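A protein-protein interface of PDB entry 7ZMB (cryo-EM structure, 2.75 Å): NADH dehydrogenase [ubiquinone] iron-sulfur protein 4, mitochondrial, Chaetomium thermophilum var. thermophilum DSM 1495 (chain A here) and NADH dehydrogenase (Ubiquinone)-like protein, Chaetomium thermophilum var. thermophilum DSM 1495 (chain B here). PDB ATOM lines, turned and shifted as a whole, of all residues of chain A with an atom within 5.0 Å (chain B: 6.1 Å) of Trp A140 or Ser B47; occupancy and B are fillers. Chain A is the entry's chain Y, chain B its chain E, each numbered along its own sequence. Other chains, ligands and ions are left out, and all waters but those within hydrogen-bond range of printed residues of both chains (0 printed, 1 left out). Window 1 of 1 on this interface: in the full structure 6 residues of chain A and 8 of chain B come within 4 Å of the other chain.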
ATOM      1  N   PHE A  74      -2.853 -13.181 -25.937  1.00  0.00           N
ATOM      2  CA  PHE A  74      -4.205 -13.052 -26.460  1.00  0.00           C
ATOM      3  C   PHE A  74      -4.879 -11.767 -25.993  1.00  0.00           C
ATOM      4  O   PHE A  74      -6.090 -11.611 -26.165  1.00  0.00           O
ATOM      5  CB  PHE A  74      -5.064 -14.254 -26.065  1.00  0.00           C
ATOM      6  CG  PHE A  74      -4.415 -15.576 -26.309  1.00  0.00           C
ATOM      7  CD1 PHE A  74      -4.470 -16.172 -27.555  1.00  0.00           C
ATOM      8  CD2 PHE A  74      -3.772 -16.239 -25.284  1.00  0.00           C
ATOM      9  CE1 PHE A  74      -3.882 -17.387 -27.778  1.00  0.00           C
ATOM     10  CE2 PHE A  74      -3.189 -17.457 -25.501  1.00  0.00           C
ATOM     11  CZ  PHE A  74      -3.243 -18.032 -26.751  1.00  0.00           C
ATOM     12  N   GLY A 137      -7.464 -17.894 -28.977  1.00  0.00           N
ATOM     13  CA  GLY A 137      -7.436 -18.163 -27.563  1.00  0.00           C
ATOM     14  C   GLY A 137      -8.759 -18.510 -26.920  1.00  0.00           C
ATOM     15  O   GLY A 137      -8.774 -18.827 -25.726  1.00  0.00           O
ATOM     16  N   HIS A 138      -9.874 -18.452 -27.655  1.00  0.00           N
ATOM     17  CA  HIS A 138     -11.159 -18.776 -27.043  1.00  0.00           C
ATOM     18  C   HIS A 138     -11.275 -20.266 -26.766  1.00  0.00           C
ATOM     19  O   HIS A 138     -11.718 -20.662 -25.685  1.00  0.00           O
ATOM     20  CB  HIS A 138     -12.310 -18.297 -27.922  1.00  0.00           C
ATOM     21  CG  HIS A 138     -13.664 -18.581 -27.349  1.00  0.00           C
ATOM     22  ND1 HIS A 138     -14.578 -19.403 -27.969  1.00  0.00           N
ATOM     23  CD2 HIS A 138     -14.259 -18.151 -26.211  1.00  0.00           C
ATOM     24  CE1 HIS A 138     -15.675 -19.468 -27.238  1.00  0.00           C
ATOM     25  NE2 HIS A 138     -15.506 -18.719 -26.166  1.00  0.00           N
ATOM     26  N   ARG A 139     -10.879 -21.103 -27.722  1.00  0.00           N
ATOM     27  CA  ARG A 139     -10.843 -22.548 -27.543  1.00  0.00           C
ATOM     28  C   ARG A 139      -9.744 -23.124 -28.418  1.00  0.00           C
ATOM     29  O   ARG A 139      -9.507 -22.654 -29.530  1.00  0.00           O
ATOM     30  CB  ARG A 139     -12.175 -23.227 -27.901  1.00  0.00           C
ATOM     31  CG  ARG A 139     -13.340 -22.971 -26.973  1.00  0.00           C
ATOM     32  CD  ARG A 139     -13.127 -23.565 -25.598  1.00  0.00           C
ATOM     33  NE  ARG A 139     -14.343 -23.515 -24.799  1.00  0.00           N
ATOM     34  CZ  ARG A 139     -14.783 -22.438 -24.164  1.00  0.00           C
ATOM     35  NH1 ARG A 139     -15.904 -22.490 -23.471  1.00  0.00           N
ATOM     36  NH2 ARG A 139     -14.107 -21.309 -24.221  1.00  0.00           N
ATOM     37  N   TRP A 140      -9.081 -24.150 -27.899  1.00  0.00           N
ATOM     38  CA  TRP A 140      -8.207 -25.011 -28.679  1.00  0.00           C
ATOM     39  C   TRP A 140      -8.197 -26.368 -27.992  1.00  0.00           C
ATOM     40  O   TRP A 140      -8.557 -26.487 -26.821  1.00  0.00           O
ATOM     41  CB  TRP A 140      -6.792 -24.430 -28.822  1.00  0.00           C
ATOM     42  CG  TRP A 140      -5.952 -24.458 -27.575  1.00  0.00           C
ATOM     43  CD1 TRP A 140      -5.187 -25.489 -27.120  1.00  0.00           C
ATOM     44  CD2 TRP A 140      -5.796 -23.402 -26.629  1.00  0.00           C
ATOM     45  NE1 TRP A 140      -4.565 -25.142 -25.955  1.00  0.00           N
ATOM     46  CE2 TRP A 140      -4.921 -23.864 -25.629  1.00  0.00           C
ATOM     47  CE3 TRP A 140      -6.313 -22.108 -26.525  1.00  0.00           C
ATOM     48  CZ2 TRP A 140      -4.553 -23.078 -24.538  1.00  0.00           C
ATOM     49  CZ3 TRP A 140      -5.947 -21.334 -25.449  1.00  0.00           C
ATOM     50  CH2 TRP A 140      -5.076 -21.818 -24.470  1.00  0.00           C
ATOM     51  N   GLU A 141      -7.860 -27.396 -28.776  1.00  0.00           N
ATOM     52  CA  GLU A 141      -7.925 -28.791 -28.282  1.00  0.00           C
ATOM     53  C   GLU A 141      -6.646 -29.228 -27.572  1.00  0.00           C
ATOM     54  O   GLU A 141      -5.567 -29.072 -28.149  1.00  0.00           O
ATOM     55  CB  GLU A 141      -8.257 -29.711 -29.453  1.00  0.00           C
ATOM     56  CG  GLU A 141      -8.408 -31.167 -29.077  1.00  0.00           C
ATOM     57  CD  GLU A 141      -8.241 -32.105 -30.256  1.00  0.00           C
ATOM     58  OE1 GLU A 141      -7.701 -31.662 -31.288  1.00  0.00           O
ATOM     59  OE2 GLU A 141      -8.650 -33.270 -30.140  1.00  0.00           O
ATOM     60  N   ASN A 142      -6.787 -29.748 -26.355  1.00  0.00           N
ATOM     61  CA  ASN A 142      -5.664 -30.265 -25.586  1.00  0.00           C
ATOM     62  C   ASN A 142      -5.049 -31.462 -26.302  1.00  0.00           C
ATOM     63  O   ASN A 142      -5.780 -32.358 -26.738  1.00  0.00           O
ATOM     64  CB  ASN A 142      -6.150 -30.665 -24.193  1.00  0.00           C
ATOM     65  CG  ASN A 142      -5.033 -31.113 -23.265  1.00  0.00           C
ATOM     66  OD1 ASN A 142      -5.099 -32.160 -22.626  1.00  0.00           O
ATOM     67  ND2 ASN A 142      -3.984 -30.312 -23.207  1.00  0.00           N
ATOM     68  N   TRP A 147      -9.736 -32.518 -24.587  1.00  0.00           N
ATOM     69  CA  TRP A 147     -10.523 -31.506 -23.907  1.00  0.00           C
ATOM     70  C   TRP A 147     -10.260 -30.140 -24.528  1.00  0.00           C
ATOM     71  O   TRP A 147      -9.227 -29.900 -25.157  1.00  0.00           O
ATOM     72  CB  TRP A 147     -10.191 -31.452 -22.416  1.00  0.00           C
ATOM     73  CG  TRP A 147     -10.468 -32.699 -21.662  1.00  0.00           C
ATOM     74  CD1 TRP A 147     -11.329 -33.693 -22.007  1.00  0.00           C
ATOM     75  CD2 TRP A 147      -9.872 -33.094 -20.429  1.00  0.00           C
ATOM     76  NE1 TRP A 147     -11.305 -34.684 -21.064  1.00  0.00           N
ATOM     77  CE2 TRP A 147     -10.417 -34.339 -20.084  1.00  0.00           C
ATOM     78  CE3 TRP A 147      -8.920 -32.518 -19.587  1.00  0.00           C
ATOM     79  CZ2 TRP A 147     -10.043 -35.020 -18.926  1.00  0.00           C
ATOM     80  CZ3 TRP A 147      -8.553 -33.191 -18.445  1.00  0.00           C
ATOM     81  CH2 TRP A 147      -9.113 -34.424 -18.120  1.00  0.00           C
ATOM     82  N   GLN A 148     -11.202 -29.236 -24.341  1.00  0.00           N
ATOM     83  CA  GLN A 148     -11.133 -27.928 -24.970  1.00  0.00           C
ATOM     84  C   GLN A 148     -10.566 -26.923 -23.981  1.00  0.00           C
ATOM     85  O   GLN A 148     -11.204 -26.584 -22.982  1.00  0.00           O
ATOM     86  CB  GLN A 148     -12.504 -27.520 -25.485  1.00  0.00           C
ATOM     87  CG  GLN A 148     -12.952 -28.413 -26.610  1.00  0.00           C
ATOM     88  CD  GLN A 148     -14.292 -28.038 -27.106  1.00  0.00           C
ATOM     89  OE1 GLN A 148     -14.918 -27.146 -26.562  1.00  0.00           O
ATOM     90  NE2 GLN A 148     -14.755 -28.710 -28.136  1.00  0.00           N
ATOM     91  N   SER A 149      -9.359 -26.458 -24.272  1.00  0.00           N
ATOM     92  CA  SER A 149      -8.624 -25.496 -23.479  1.00  0.00           C
ATOM     93  C   SER A 149      -9.090 -24.082 -23.809  1.00  0.00           C
ATOM     94  O   SER A 149      -9.845 -23.855 -24.754  1.00  0.00           O
ATOM     95  CB  SER A 149      -7.133 -25.642 -23.744  1.00  0.00           C
ATOM     96  OG  SER A 149      -6.691 -26.953 -23.465  1.00  0.00           O
ATOM     97  N   SER A 150      -8.639 -23.119 -23.011  1.00  0.00           N
ATOM     98  CA  SER A 150      -9.035 -21.737 -23.239  1.00  0.00           C
ATOM     99  C   SER A 150      -8.063 -20.794 -22.549  1.00  0.00           C
ATOM    100  O   SER A 150      -7.463 -21.129 -21.529  1.00  0.00           O
ATOM    101  CB  SER A 150     -10.461 -21.473 -22.749  1.00  0.00           C
ATOM    102  OG  SER A 150     -11.004 -20.314 -23.340  1.00  0.00           O
ATOM    103  N   ALA A 151      -7.919 -19.611 -23.134  1.00  0.00           N
ATOM    104  CA  ALA A 151      -7.150 -18.525 -22.544  1.00  0.00           C
ATOM    105  C   ALA A 151      -7.998 -17.280 -22.331  1.00  0.00           C
ATOM    106  O   ALA A 151      -7.464 -16.239 -21.948  1.00  0.00           O
ATOM    107  CB  ALA A 151      -5.937 -18.197 -23.412  1.00  0.00           C
ATOM    108  N   ILE B  41      -0.359 -22.197 -31.017  1.00  0.00           N
ATOM    109  CA  ILE B  41      -0.978 -21.282 -30.061  1.00  0.00           C
ATOM    110  C   ILE B  41       0.067 -21.012 -28.988  1.00  0.00           C
ATOM    111  O   ILE B  41       0.639 -21.951 -28.424  1.00  0.00           O
ATOM    112  CB  ILE B  41      -2.275 -21.857 -29.470  1.00  0.00           C
ATOM    113  CG1 ILE B  41      -3.353 -22.012 -30.542  1.00  0.00           C
ATOM    114  CG2 ILE B  41      -2.785 -20.995 -28.355  1.00  0.00           C
ATOM    115  CD1 ILE B  41      -3.358 -23.296 -31.253  1.00  0.00           C
ATOM    116  N   GLN B  42       0.319 -19.736 -28.699  1.00  0.00           N
ATOM    117  CA  GLN B  42       1.628 -19.361 -28.176  1.00  0.00           C
ATOM    118  C   GLN B  42       1.770 -19.610 -26.677  1.00  0.00           C
ATOM    119  O   GLN B  42       2.594 -20.428 -26.251  1.00  0.00           O
ATOM    120  CB  GLN B  42       1.914 -17.902 -28.506  1.00  0.00           C
ATOM    121  CG  GLN B  42       1.704 -17.561 -29.968  1.00  0.00           C
ATOM    122  CD  GLN B  42       2.806 -18.089 -30.869  1.00  0.00           C
ATOM    123  OE1 GLN B  42       3.327 -19.183 -30.660  1.00  0.00           O
ATOM    124  NE2 GLN B  42       3.171 -17.304 -31.877  1.00  0.00           N
ATOM    125  N   GLY B  43       1.010 -18.914 -25.864  1.00  0.00           N
ATOM    126  CA  GLY B  43       1.405 -18.734 -24.486  1.00  0.00           C
ATOM    127  C   GLY B  43       1.040 -19.879 -23.572  1.00  0.00           C
ATOM    128  O   GLY B  43       0.121 -20.632 -23.834  1.00  0.00           O
ATOM    129  N   GLY B  44       1.783 -20.005 -22.479  1.00  0.00           N
ATOM    130  CA  GLY B  44       1.381 -20.858 -21.381  1.00  0.00           C
ATOM    131  C   GLY B  44       1.733 -22.317 -21.579  1.00  0.00           C
ATOM    132  O   GLY B  44       2.131 -22.763 -22.654  1.00  0.00           O
ATOM    133  N   ARG B  45       1.588 -23.076 -20.491  1.00  0.00           N
ATOM    134  CA  ARG B  45       1.860 -24.507 -20.514  1.00  0.00           C
ATOM    135  C   ARG B  45       0.672 -25.320 -20.999  1.00  0.00           C
ATOM    136  O   ARG B  45       0.829 -26.516 -21.251  1.00  0.00           O
ATOM    137  CB  ARG B  45       2.297 -24.995 -19.122  1.00  0.00           C
ATOM    138  CG  ARG B  45       1.278 -24.805 -18.010  1.00  0.00           C
ATOM    139  CD  ARG B  45       1.886 -25.050 -16.643  1.00  0.00           C
ATOM    140  NE  ARG B  45       2.055 -26.449 -16.271  1.00  0.00           N
ATOM    141  CZ  ARG B  45       2.905 -26.858 -15.334  1.00  0.00           C
ATOM    142  NH1 ARG B  45       3.008 -28.136 -15.020  1.00  0.00           N
ATOM    143  NH2 ARG B  45       3.678 -25.979 -14.724  1.00  0.00           N
ATOM    144  N   SER B  46      -0.495 -24.704 -21.149  1.00  0.00           N
ATOM    145  CA  SER B  46      -1.671 -25.376 -21.679  1.00  0.00           C
ATOM    146  C   SER B  46      -1.800 -25.252 -23.191  1.00  0.00           C
ATOM    147  O   SER B  46      -2.713 -25.846 -23.765  1.00  0.00           O
ATOM    148  CB  SER B  46      -2.937 -24.828 -21.020  1.00  0.00           C
ATOM    149  OG  SER B  46      -2.874 -24.920 -19.614  1.00  0.00           O
ATOM    150  N   SER B  47      -0.914 -24.516 -23.846  1.00  0.00           N
ATOM    151  CA  SER B  47      -1.068 -24.219 -25.261  1.00  0.00           C
ATOM    152  C   SER B  47      -0.317 -25.224 -26.130  1.00  0.00           C
ATOM    153  O   SER B  47       0.135 -26.273 -25.672  1.00  0.00           O
ATOM    154  CB  SER B  47      -0.621 -22.795 -25.548  1.00  0.00           C
ATOM    155  OG  SER B  47       0.743 -22.617 -25.225  1.00  0.00           O
ATOM    156  N   LEU B  48      -0.181 -24.894 -27.410  1.00  0.00           N
ATOM    157  CA  LEU B  48       0.309 -25.807 -28.438  1.00  0.00           C
ATOM    158  C   LEU B  48       1.574 -25.224 -29.061  1.00  0.00           C
ATOM    159  O   LEU B  48       1.504 -24.320 -29.895  1.00  0.00           O
ATOM    160  CB  LEU B  48      -0.770 -26.042 -29.491  1.00  0.00           C
ATOM    161  CG  LEU B  48      -2.148 -26.403 -28.943  1.00  0.00           C
ATOM    162  CD1 LEU B  48      -3.169 -26.556 -30.047  1.00  0.00           C
ATOM    163  CD2 LEU B  48      -2.059 -27.672 -28.140  1.00  0.00           C
ATOM    164  N   GLY B  49       2.727 -25.750 -28.667  1.00  0.00           N
ATOM    165  CA  GLY B  49       3.988 -25.351 -29.251  1.00  0.00           C
ATOM    166  C   GLY B  49       4.339 -26.157 -30.478  1.00  0.00           C
ATOM    167  O   GLY B  49       5.217 -25.771 -31.253  1.00  0.00           O
ATOM    168  N   ARG B  72       7.462 -25.086 -21.130  1.00  0.00           N
ATOM    169  CA  ARG B  72       6.508 -24.098 -20.645  1.00  0.00           C
ATOM    170  C   ARG B  72       5.811 -23.362 -21.774  1.00  0.00           C
ATOM    171  O   ARG B  72       4.877 -22.601 -21.509  1.00  0.00           O
ATOM    172  CB  ARG B  72       7.190 -23.092 -19.717  1.00  0.00           C
ATOM    173  CG  ARG B  72       8.070 -22.103 -20.414  1.00  0.00           C
ATOM    174  CD  ARG B  72       9.180 -21.631 -19.523  1.00  0.00           C
ATOM    175  NE  ARG B  72      10.246 -21.027 -20.312  1.00  0.00           N
ATOM    176  CZ  ARG B  72      10.427 -19.721 -20.457  1.00  0.00           C
ATOM    177  NH1 ARG B  72       9.614 -18.867 -19.853  1.00  0.00           N
ATOM    178  NH2 ARG B  72      11.422 -19.272 -21.205  1.00  0.00           N
ATOM    179  N   GLN B  73       6.258 -23.550 -23.015  1.00  0.00           N
ATOM    180  CA  GLN B  73       5.543 -23.085 -24.195  1.00  0.00           C
ATOM    181  C   GLN B  73       4.802 -24.213 -24.895  1.00  0.00           C
ATOM    182  O   GLN B  73       4.570 -24.143 -26.104  1.00  0.00           O
ATOM    183  CB  GLN B  73       6.499 -22.401 -25.165  1.00  0.00           C
ATOM    184  CG  GLN B  73       7.451 -21.458 -24.499  1.00  0.00           C
ATOM    185  CD  GLN B  73       8.297 -20.712 -25.491  1.00  0.00           C
ATOM    186  OE1 GLN B  73       8.012 -20.708 -26.685  1.00  0.00           O
ATOM    187  NE2 GLN B  73       9.348 -20.070 -25.004  1.00  0.00           N
ATOM    188  N   GLY B  74       4.440 -25.259 -24.158  1.00  0.00           N
ATOM    189  CA  GLY B  74       3.594 -26.314 -24.676  1.00  0.00           C
ATOM    190  C   GLY B  74       4.183 -27.167 -25.777  1.00  0.00           C
ATOM    191  O   GLY B  74       3.513 -27.442 -26.773  1.00  0.00           O
ATOM    192  N   CYS B  75       5.426 -27.592 -25.619  1.00  0.00           N
ATOM    193  CA  CYS B  75       6.058 -28.517 -26.544  1.00  0.00           C
ATOM    194  C   CYS B  75       6.310 -29.846 -25.848  1.00  0.00           C
ATOM    195  O   CYS B  75       6.640 -29.884 -24.660  1.00  0.00           O
ATOM    196  CB  CYS B  75       7.372 -27.949 -27.083  1.00  0.00           C
ATOM    197  SG  CYS B  75       7.168 -26.564 -28.219  1.00  0.00           S
ATOM    198  N   ARG B  98       3.268 -33.654 -21.311  1.00  0.00           N
ATOM    199  CA  ARG B  98       4.208 -32.855 -22.083  1.00  0.00           C
ATOM    200  C   ARG B  98       5.630 -33.381 -21.991  1.00  0.00           C
ATOM    201  O   ARG B  98       6.306 -33.522 -23.010  1.00  0.00           O
ATOM    202  CB  ARG B  98       4.155 -31.398 -21.620  1.00  0.00           C
ATOM    203  CG  ARG B  98       3.051 -30.616 -22.281  1.00  0.00           C
ATOM    204  CD  ARG B  98       3.145 -30.778 -23.773  1.00  0.00           C
ATOM    205  NE  ARG B  98       2.342 -29.796 -24.480  1.00  0.00           N
ATOM    206  CZ  ARG B  98       1.875 -29.972 -25.706  1.00  0.00           C
ATOM    207  NH1 ARG B  98       1.155 -29.025 -26.282  1.00  0.00           N
ATOM    208  NH2 ARG B  98       2.141 -31.095 -26.355  1.00  0.00           N
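The backbone carbonyl oxygen (O) of Ser B46 is in hydrogen-bond range of the indole nitrogen (NE1) of Trp A140 (3.0 Å).
The backbone carbonyl oxygen of Leu B48 is in hydrogen-bond range of the backbone NH of Ile B41.
The backbone carbonyl oxygen (O) of Gln B42 is in hydrogen-bond range of the side-chain hydroxyl (OG) of Ser B47, 3.0 Å away.
O of Gly B43 is in hydrogen-bond range of OG of Ser B47.
The side-chain hydroxyl (OG) of Ser B47 is in hydrogen-bond range of the backbone carbonyl oxygen (O) of Gly B44 (2.9 Å).
The backbone carbonyl oxygen of Ser B47 is in hydrogen-bond range of the guanidinium group of Arg B98 (3.0 Å).
O of Trp A140 is in hydrogen-bond range of N of Ser A149.
Among the printed residues, merely in contact across the chains: Phe A74 with Ile B41, Trp A140 with Leu B48, Trp A140 with Ser B47 and Glu A141 with Leu B48.
Of chain B, only Ser B46, Ser B47 and Leu B48 come within 4 Å of Trp A140.
Ser B47 touches just one residue of chain A: Trp A140 (3.7 Å).
Of the printed residues of chain A, Ser B46 touches Trp A140.
Printed residues of chain A within 4 Å of Ile B41: Phe A74.
Of the printed residues of chain B, Phe A74 touches Ile B41 (3.4 Å).
Of the printed residues of chain A, Leu B48 touches Trp A140 (3.7 Å) and Glu A141 (3.8 Å).
Gly B43 touches none of the printed residues of chain A.
Gln B73 touches none of the printed residues of chain A.
The nearest printed residue of chain A that does not touch Ser B47 is Phe A74 (5.6 Å).
The nearest printed residue of chain B that does not touch Glu A141 is Ser B46 (6.1 Å).
Printed residues of chain B that touch a printed residue of chain A: Ile B41, Ser B46, Ser B47 and Leu B48.
Hydrophobic or aromatic side chains of chain B within 4 Å of the printed part of chain A: Ile B41 and Leu B48.
Printed residues of chain A that touch a printed residue of chain B: Phe A74, Trp A140 and Glu A141.
Among the printed residues, 5 pairs touch across the chains.
Among the printed residues, no Asp or Glu carboxylate lies within 4 Å of a Lys or Arg side-chain nitrogen of the other chain.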
